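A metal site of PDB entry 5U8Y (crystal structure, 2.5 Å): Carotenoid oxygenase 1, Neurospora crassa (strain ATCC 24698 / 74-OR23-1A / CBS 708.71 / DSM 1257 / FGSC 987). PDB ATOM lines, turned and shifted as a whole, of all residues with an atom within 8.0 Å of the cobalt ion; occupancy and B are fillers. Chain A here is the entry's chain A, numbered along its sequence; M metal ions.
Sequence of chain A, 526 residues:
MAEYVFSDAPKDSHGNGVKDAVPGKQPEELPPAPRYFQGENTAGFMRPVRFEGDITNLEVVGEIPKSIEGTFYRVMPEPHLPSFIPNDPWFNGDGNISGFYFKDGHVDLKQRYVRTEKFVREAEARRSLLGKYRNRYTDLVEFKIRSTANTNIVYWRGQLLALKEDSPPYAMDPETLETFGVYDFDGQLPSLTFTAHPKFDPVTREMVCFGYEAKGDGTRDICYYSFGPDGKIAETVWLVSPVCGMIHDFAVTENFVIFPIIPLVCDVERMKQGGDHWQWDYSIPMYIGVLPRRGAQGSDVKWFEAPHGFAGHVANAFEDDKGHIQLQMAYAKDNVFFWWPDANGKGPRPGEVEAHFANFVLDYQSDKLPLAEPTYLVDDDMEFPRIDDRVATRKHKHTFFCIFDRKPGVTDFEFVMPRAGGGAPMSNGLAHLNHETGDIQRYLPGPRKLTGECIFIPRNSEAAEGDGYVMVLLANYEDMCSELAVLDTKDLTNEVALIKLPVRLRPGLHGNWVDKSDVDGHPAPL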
ATOM      1  N   PHE A  91     -26.538  21.097 -14.960  1.00  0.00           N
ATOM      2  CA  PHE A  91     -27.025  21.938 -13.833  1.00  0.00           C
ATOM      3  C   PHE A  91     -28.355  22.673 -14.036  1.00  0.00           C
ATOM      4  O   PHE A  91     -28.854  23.277 -13.065  1.00  0.00           O
ATOM      5  CB  PHE A  91     -25.996  23.042 -13.471  1.00  0.00           C
ATOM      6  CG  PHE A  91     -24.729  22.563 -12.850  1.00  0.00           C
ATOM      7  CD1 PHE A  91     -24.629  21.254 -12.354  1.00  0.00           C
ATOM      8  CD2 PHE A  91     -23.613  23.382 -12.805  1.00  0.00           C
ATOM      9  CE1 PHE A  91     -23.445  20.809 -11.779  1.00  0.00           C
ATOM     10  CE2 PHE A  91     -22.423  22.933 -12.249  1.00  0.00           C
ATOM     11  CZ  PHE A  91     -22.348  21.649 -11.723  1.00  0.00           C
ATOM     12  N   THR A 151     -30.076  20.868  -6.648  1.00  0.00           N
ATOM     13  CA  THR A 151     -28.677  20.729  -6.221  1.00  0.00           C
ATOM     14  C   THR A 151     -28.550  19.941  -4.917  1.00  0.00           C
ATOM     15  O   THR A 151     -27.678  19.118  -4.791  1.00  0.00           O
ATOM     16  CB  THR A 151     -27.996  22.116  -6.079  1.00  0.00           C
ATOM     17  OG1 THR A 151     -28.169  22.858  -7.291  1.00  0.00           O
ATOM     18  CG2 THR A 151     -26.514  21.988  -5.778  1.00  0.00           C
ATOM     19  N   ASN A 152     -29.403  20.234  -3.950  1.00  0.00           N
ATOM     20  CA  ASN A 152     -29.368  19.504  -2.678  1.00  0.00           C
ATOM     21  C   ASN A 152     -30.767  19.433  -2.101  1.00  0.00           C
ATOM     22  O   ASN A 152     -31.670  20.179  -2.510  1.00  0.00           O
ATOM     23  CB  ASN A 152     -28.406  20.200  -1.699  1.00  0.00           C
ATOM     24  CG  ASN A 152     -27.918  19.291  -0.582  1.00  0.00           C
ATOM     25  OD1 ASN A 152     -28.288  18.113  -0.496  1.00  0.00           O
ATOM     26  ND2 ASN A 152     -27.076  19.826   0.286  1.00  0.00           N
ATOM     27  N   GLU A 165     -28.744  27.524  -5.635  1.00  0.00           N
ATOM     28  CA  GLU A 165     -28.058  28.713  -5.114  1.00  0.00           C
ATOM     29  C   GLU A 165     -28.412  30.080  -5.718  1.00  0.00           C
ATOM     30  O   GLU A 165     -27.941  31.112  -5.200  1.00  0.00           O
ATOM     31  CB  GLU A 165     -26.544  28.502  -5.203  1.00  0.00           C
ATOM     32  CG  GLU A 165     -25.969  28.494  -6.615  1.00  0.00           C
ATOM     33  CD  GLU A 165     -24.673  27.727  -6.728  1.00  0.00           C
ATOM     34  OE1 GLU A 165     -23.746  28.303  -7.369  1.00  0.00           O
ATOM     35  OE2 GLU A 165     -24.568  26.598  -6.195  1.00  0.00           O
ATOM     36  N   THR A 195     -27.838  29.192  -0.177  1.00  0.00           N
ATOM     37  CA  THR A 195     -26.825  28.247  -0.612  1.00  0.00           C
ATOM     38  C   THR A 195     -27.350  26.812  -0.691  1.00  0.00           C
ATOM     39  O   THR A 195     -28.246  26.419   0.048  1.00  0.00           O
ATOM     40  CB  THR A 195     -25.580  28.262   0.311  1.00  0.00           C
ATOM     41  OG1 THR A 195     -24.583  27.351  -0.180  1.00  0.00           O
ATOM     42  CG2 THR A 195     -25.930  27.852   1.740  1.00  0.00           C
ATOM     43  N   ALA A 196     -26.779  26.038  -1.601  1.00  0.00           N
ATOM     44  CA  ALA A 196     -27.044  24.625  -1.632  1.00  0.00           C
ATOM     45  C   ALA A 196     -26.313  23.847  -0.551  1.00  0.00           C
ATOM     46  O   ALA A 196     -26.546  22.666  -0.419  1.00  0.00           O
ATOM     47  CB  ALA A 196     -26.687  24.062  -2.992  1.00  0.00           C
ATOM     48  N   HIS A 197     -25.430  24.497   0.208  1.00  0.00           N
ATOM     49  CA  HIS A 197     -24.620  23.809   1.220  1.00  0.00           C
ATOM     50  C   HIS A 197     -24.662  24.467   2.588  1.00  0.00           C
ATOM     51  O   HIS A 197     -23.619  24.855   3.135  1.00  0.00           O
ATOM     52  CB  HIS A 197     -23.199  23.709   0.731  1.00  0.00           C
ATOM     53  CG  HIS A 197     -23.056  22.758  -0.399  1.00  0.00           C
ATOM     54  ND1 HIS A 197     -23.120  21.406  -0.205  1.00  0.00           N
ATOM     55  CD2 HIS A 197     -22.937  22.939  -1.734  1.00  0.00           C
ATOM     56  CE1 HIS A 197     -23.027  20.787  -1.360  1.00  0.00           C
ATOM     57  NE2 HIS A 197     -22.910  21.701  -2.311  1.00  0.00           N
ATOM     58  N   HIS A 248     -19.948  28.306  -4.236  1.00  0.00           N
ATOM     59  CA  HIS A 248     -20.818  27.150  -4.222  1.00  0.00           C
ATOM     60  C   HIS A 248     -20.995  26.547  -2.844  1.00  0.00           C
ATOM     61  O   HIS A 248     -22.095  26.175  -2.446  1.00  0.00           O
ATOM     62  CB  HIS A 248     -20.287  26.075  -5.121  1.00  0.00           C
ATOM     63  CG  HIS A 248     -21.203  24.887  -5.223  1.00  0.00           C
ATOM     64  ND1 HIS A 248     -22.507  25.007  -5.668  1.00  0.00           N
ATOM     65  CD2 HIS A 248     -21.009  23.573  -4.953  1.00  0.00           C
ATOM     66  CE1 HIS A 248     -23.067  23.814  -5.695  1.00  0.00           C
ATOM     67  NE2 HIS A 248     -22.178  22.934  -5.260  1.00  0.00           N
ATOM     68  N   ASP A 249     -19.870  26.400  -2.151  1.00  0.00           N
ATOM     69  CA  ASP A 249     -19.848  25.770  -0.852  1.00  0.00           C
ATOM     70  C   ASP A 249     -19.240  26.773   0.104  1.00  0.00           C
ATOM     71  O   ASP A 249     -18.688  27.789  -0.338  1.00  0.00           O
ATOM     72  CB  ASP A 249     -19.029  24.468  -0.927  1.00  0.00           C
ATOM     73  CG  ASP A 249     -19.389  23.457   0.147  1.00  0.00           C
ATOM     74  OD1 ASP A 249     -19.974  23.825   1.197  1.00  0.00           O
ATOM     75  OD2 ASP A 249     -19.024  22.263  -0.059  1.00  0.00           O
ATOM     76  N   GLY A 312     -13.496  23.296  -4.925  1.00  0.00           N
ATOM     77  CA  GLY A 312     -14.422  22.183  -4.906  1.00  0.00           C
ATOM     78  C   GLY A 312     -15.178  22.127  -3.594  1.00  0.00           C
ATOM     79  O   GLY A 312     -15.245  23.108  -2.854  1.00  0.00           O
ATOM     80  N   HIS A 313     -15.739  20.964  -3.293  1.00  0.00           N
ATOM     81  CA  HIS A 313     -16.611  20.846  -2.123  1.00  0.00           C
ATOM     82  C   HIS A 313     -15.835  20.811  -0.838  1.00  0.00           C
ATOM     83  O   HIS A 313     -14.778  20.180  -0.758  1.00  0.00           O
ATOM     84  CB  HIS A 313     -17.494  19.604  -2.213  1.00  0.00           C
ATOM     85  CG  HIS A 313     -18.660  19.798  -3.124  1.00  0.00           C
ATOM     86  ND1 HIS A 313     -18.742  19.196  -4.362  1.00  0.00           N
ATOM     87  CD2 HIS A 313     -19.752  20.563  -3.008  1.00  0.00           C
ATOM     88  CE1 HIS A 313     -19.863  19.550  -4.961  1.00  0.00           C
ATOM     89  NE2 HIS A 313     -20.499  20.389  -4.152  1.00  0.00           N
ATOM     90  N   VAL A 314     -16.387  21.442   0.185  1.00  0.00           N
ATOM     91  CA  VAL A 314     -15.829  21.378   1.513  1.00  0.00           C
ATOM     92  C   VAL A 314     -16.193  20.054   2.194  1.00  0.00           C
ATOM     93  O   VAL A 314     -17.362  19.739   2.320  1.00  0.00           O
ATOM     94  CB  VAL A 314     -16.361  22.536   2.372  1.00  0.00           C
ATOM     95  CG1 VAL A 314     -15.882  22.423   3.803  1.00  0.00           C
ATOM     96  CG2 VAL A 314     -15.961  23.871   1.743  1.00  0.00           C
ATOM     97  N   PHE A 337     -15.328  23.406 -14.311  1.00  0.00           N
ATOM     98  CA  PHE A 337     -16.460  23.713 -15.183  1.00  0.00           C
ATOM     99  C   PHE A 337     -15.977  24.282 -16.549  1.00  0.00           C
ATOM    100  O   PHE A 337     -16.211  25.443 -16.917  1.00  0.00           O
ATOM    101  CB  PHE A 337     -17.457  24.652 -14.483  1.00  0.00           C
ATOM    102  CG  PHE A 337     -18.010  24.143 -13.153  1.00  0.00           C
ATOM    103  CD1 PHE A 337     -17.952  22.792 -12.779  1.00  0.00           C
ATOM    104  CD2 PHE A 337     -18.628  25.047 -12.277  1.00  0.00           C
ATOM    105  CE1 PHE A 337     -18.462  22.371 -11.540  1.00  0.00           C
ATOM    106  CE2 PHE A 337     -19.135  24.624 -11.047  1.00  0.00           C
ATOM    107  CZ  PHE A 337     -19.052  23.299 -10.671  1.00  0.00           C
ATOM    108  N   GLU A 383     -13.802  13.904  -5.357  1.00  0.00           N
ATOM    109  CA  GLU A 383     -14.798  14.946  -5.077  1.00  0.00           C
ATOM    110  C   GLU A 383     -15.883  14.347  -4.150  1.00  0.00           C
ATOM    111  O   GLU A 383     -15.746  13.207  -3.679  1.00  0.00           O
ATOM    112  CB  GLU A 383     -15.389  15.515  -6.389  1.00  0.00           C
ATOM    113  CG  GLU A 383     -14.970  16.994  -6.677  1.00  0.00           C
ATOM    114  CD  GLU A 383     -15.619  18.035  -5.744  1.00  0.00           C
ATOM    115  OE1 GLU A 383     -15.217  19.220  -5.714  1.00  0.00           O
ATOM    116  OE2 GLU A 383     -16.580  17.673  -5.033  1.00  0.00           O
ATOM    117  N   PHE A 384     -16.925  15.133  -3.883  1.00  0.00           N
ATOM    118  CA  PHE A 384     -18.073  14.715  -3.059  1.00  0.00           C
ATOM    119  C   PHE A 384     -17.686  14.132  -1.693  1.00  0.00           C
ATOM    120  O   PHE A 384     -18.103  13.039  -1.319  1.00  0.00           O
ATOM    121  CB  PHE A 384     -18.990  13.752  -3.857  1.00  0.00           C
ATOM    122  CG  PHE A 384     -19.642  14.370  -5.070  1.00  0.00           C
ATOM    123  CD1 PHE A 384     -20.688  15.298  -4.932  1.00  0.00           C
ATOM    124  CD2 PHE A 384     -19.222  14.044  -6.344  1.00  0.00           C
ATOM    125  CE1 PHE A 384     -21.246  15.892  -6.033  1.00  0.00           C
ATOM    126  CE2 PHE A 384     -19.811  14.607  -7.459  1.00  0.00           C
ATOM    127  CZ  PHE A 384     -20.827  15.533  -7.311  1.00  0.00           C
ATOM    128  N   GLU A 453     -22.679  10.507  -5.081  1.00  0.00           N
ATOM    129  CA  GLU A 453     -22.247  10.907  -3.748  1.00  0.00           C
ATOM    130  C   GLU A 453     -22.800   9.934  -2.712  1.00  0.00           C
ATOM    131  O   GLU A 453     -23.985   9.543  -2.768  1.00  0.00           O
ATOM    132  CB  GLU A 453     -22.786  12.304  -3.418  1.00  0.00           C
ATOM    133  CG  GLU A 453     -22.438  12.800  -2.026  1.00  0.00           C
ATOM    134  CD  GLU A 453     -23.164  14.091  -1.648  1.00  0.00           C
ATOM    135  OE1 GLU A 453     -24.404  14.055  -1.499  1.00  0.00           O
ATOM    136  OE2 GLU A 453     -22.512  15.153  -1.476  1.00  0.00           O
ATOM    137  N   LEU A 509     -26.883  14.967  -7.974  1.00  0.00           N
ATOM    138  CA  LEU A 509     -26.025  15.793  -7.176  1.00  0.00           C
ATOM    139  C   LEU A 509     -26.098  15.292  -5.733  1.00  0.00           C
ATOM    140  O   LEU A 509     -25.750  14.115  -5.496  1.00  0.00           O
ATOM    141  CB  LEU A 509     -26.436  17.269  -7.360  1.00  0.00           C
ATOM    142  CG  LEU A 509     -25.977  17.854  -8.695  1.00  0.00           C
ATOM    143  CD1 LEU A 509     -26.736  19.103  -9.105  1.00  0.00           C
ATOM    144  CD2 LEU A 509     -24.485  18.220  -8.597  1.00  0.00           C
ATOM    145  N   HIS A 510     -26.568  16.104  -4.798  1.00  0.00           N
ATOM    146  CA  HIS A 510     -26.380  15.814  -3.381  1.00  0.00           C
ATOM    147  C   HIS A 510     -27.541  15.059  -2.767  1.00  0.00           C
ATOM    148  O   HIS A 510     -28.655  15.068  -3.286  1.00  0.00           O
ATOM    149  CB  HIS A 510     -26.100  17.104  -2.607  1.00  0.00           C
ATOM    150  CG  HIS A 510     -24.851  17.798  -3.050  1.00  0.00           C
ATOM    151  ND1 HIS A 510     -23.586  17.375  -2.679  1.00  0.00           N
ATOM    152  CD2 HIS A 510     -24.663  18.846  -3.877  1.00  0.00           C
ATOM    153  CE1 HIS A 510     -22.679  18.140  -3.272  1.00  0.00           C
ATOM    154  NE2 HIS A 510     -23.316  19.049  -3.996  1.00  0.00           N
HETATM  155 CO    CO M   1     -22.523  20.992  -4.350  1.00  0.00          CO
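Within 4 Å of the cobalt ion: His 197, His 248, His 313 and His 510.
A ring nitrogen (ND1) of His 313 is in hydrogen-bond range of the side-chain carboxylate of Glu 383, 2.7 Å away.
N of His 510 lies close to O of Thr 151 (3.2 Å).
OE2 of Glu 453 sits at hydrogen-bond distance from ND1 of His 510 (2.7 Å).
OE2 of Glu 165 lies within hydrogen-bond range of ND1 of His 248 (2.7 Å).
OG1 of Thr 195 sits at hydrogen-bond distance from N of His 197.
The cobalt ion is bound by NE2 of His 313 (2.1 Å), NE2 of His 510 (2.1 Å), NE2 of His 248 (2.2 Å) and NE2 of His 197 (2.2 Å).
The cobalt ion has four donor atoms within binding distance.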
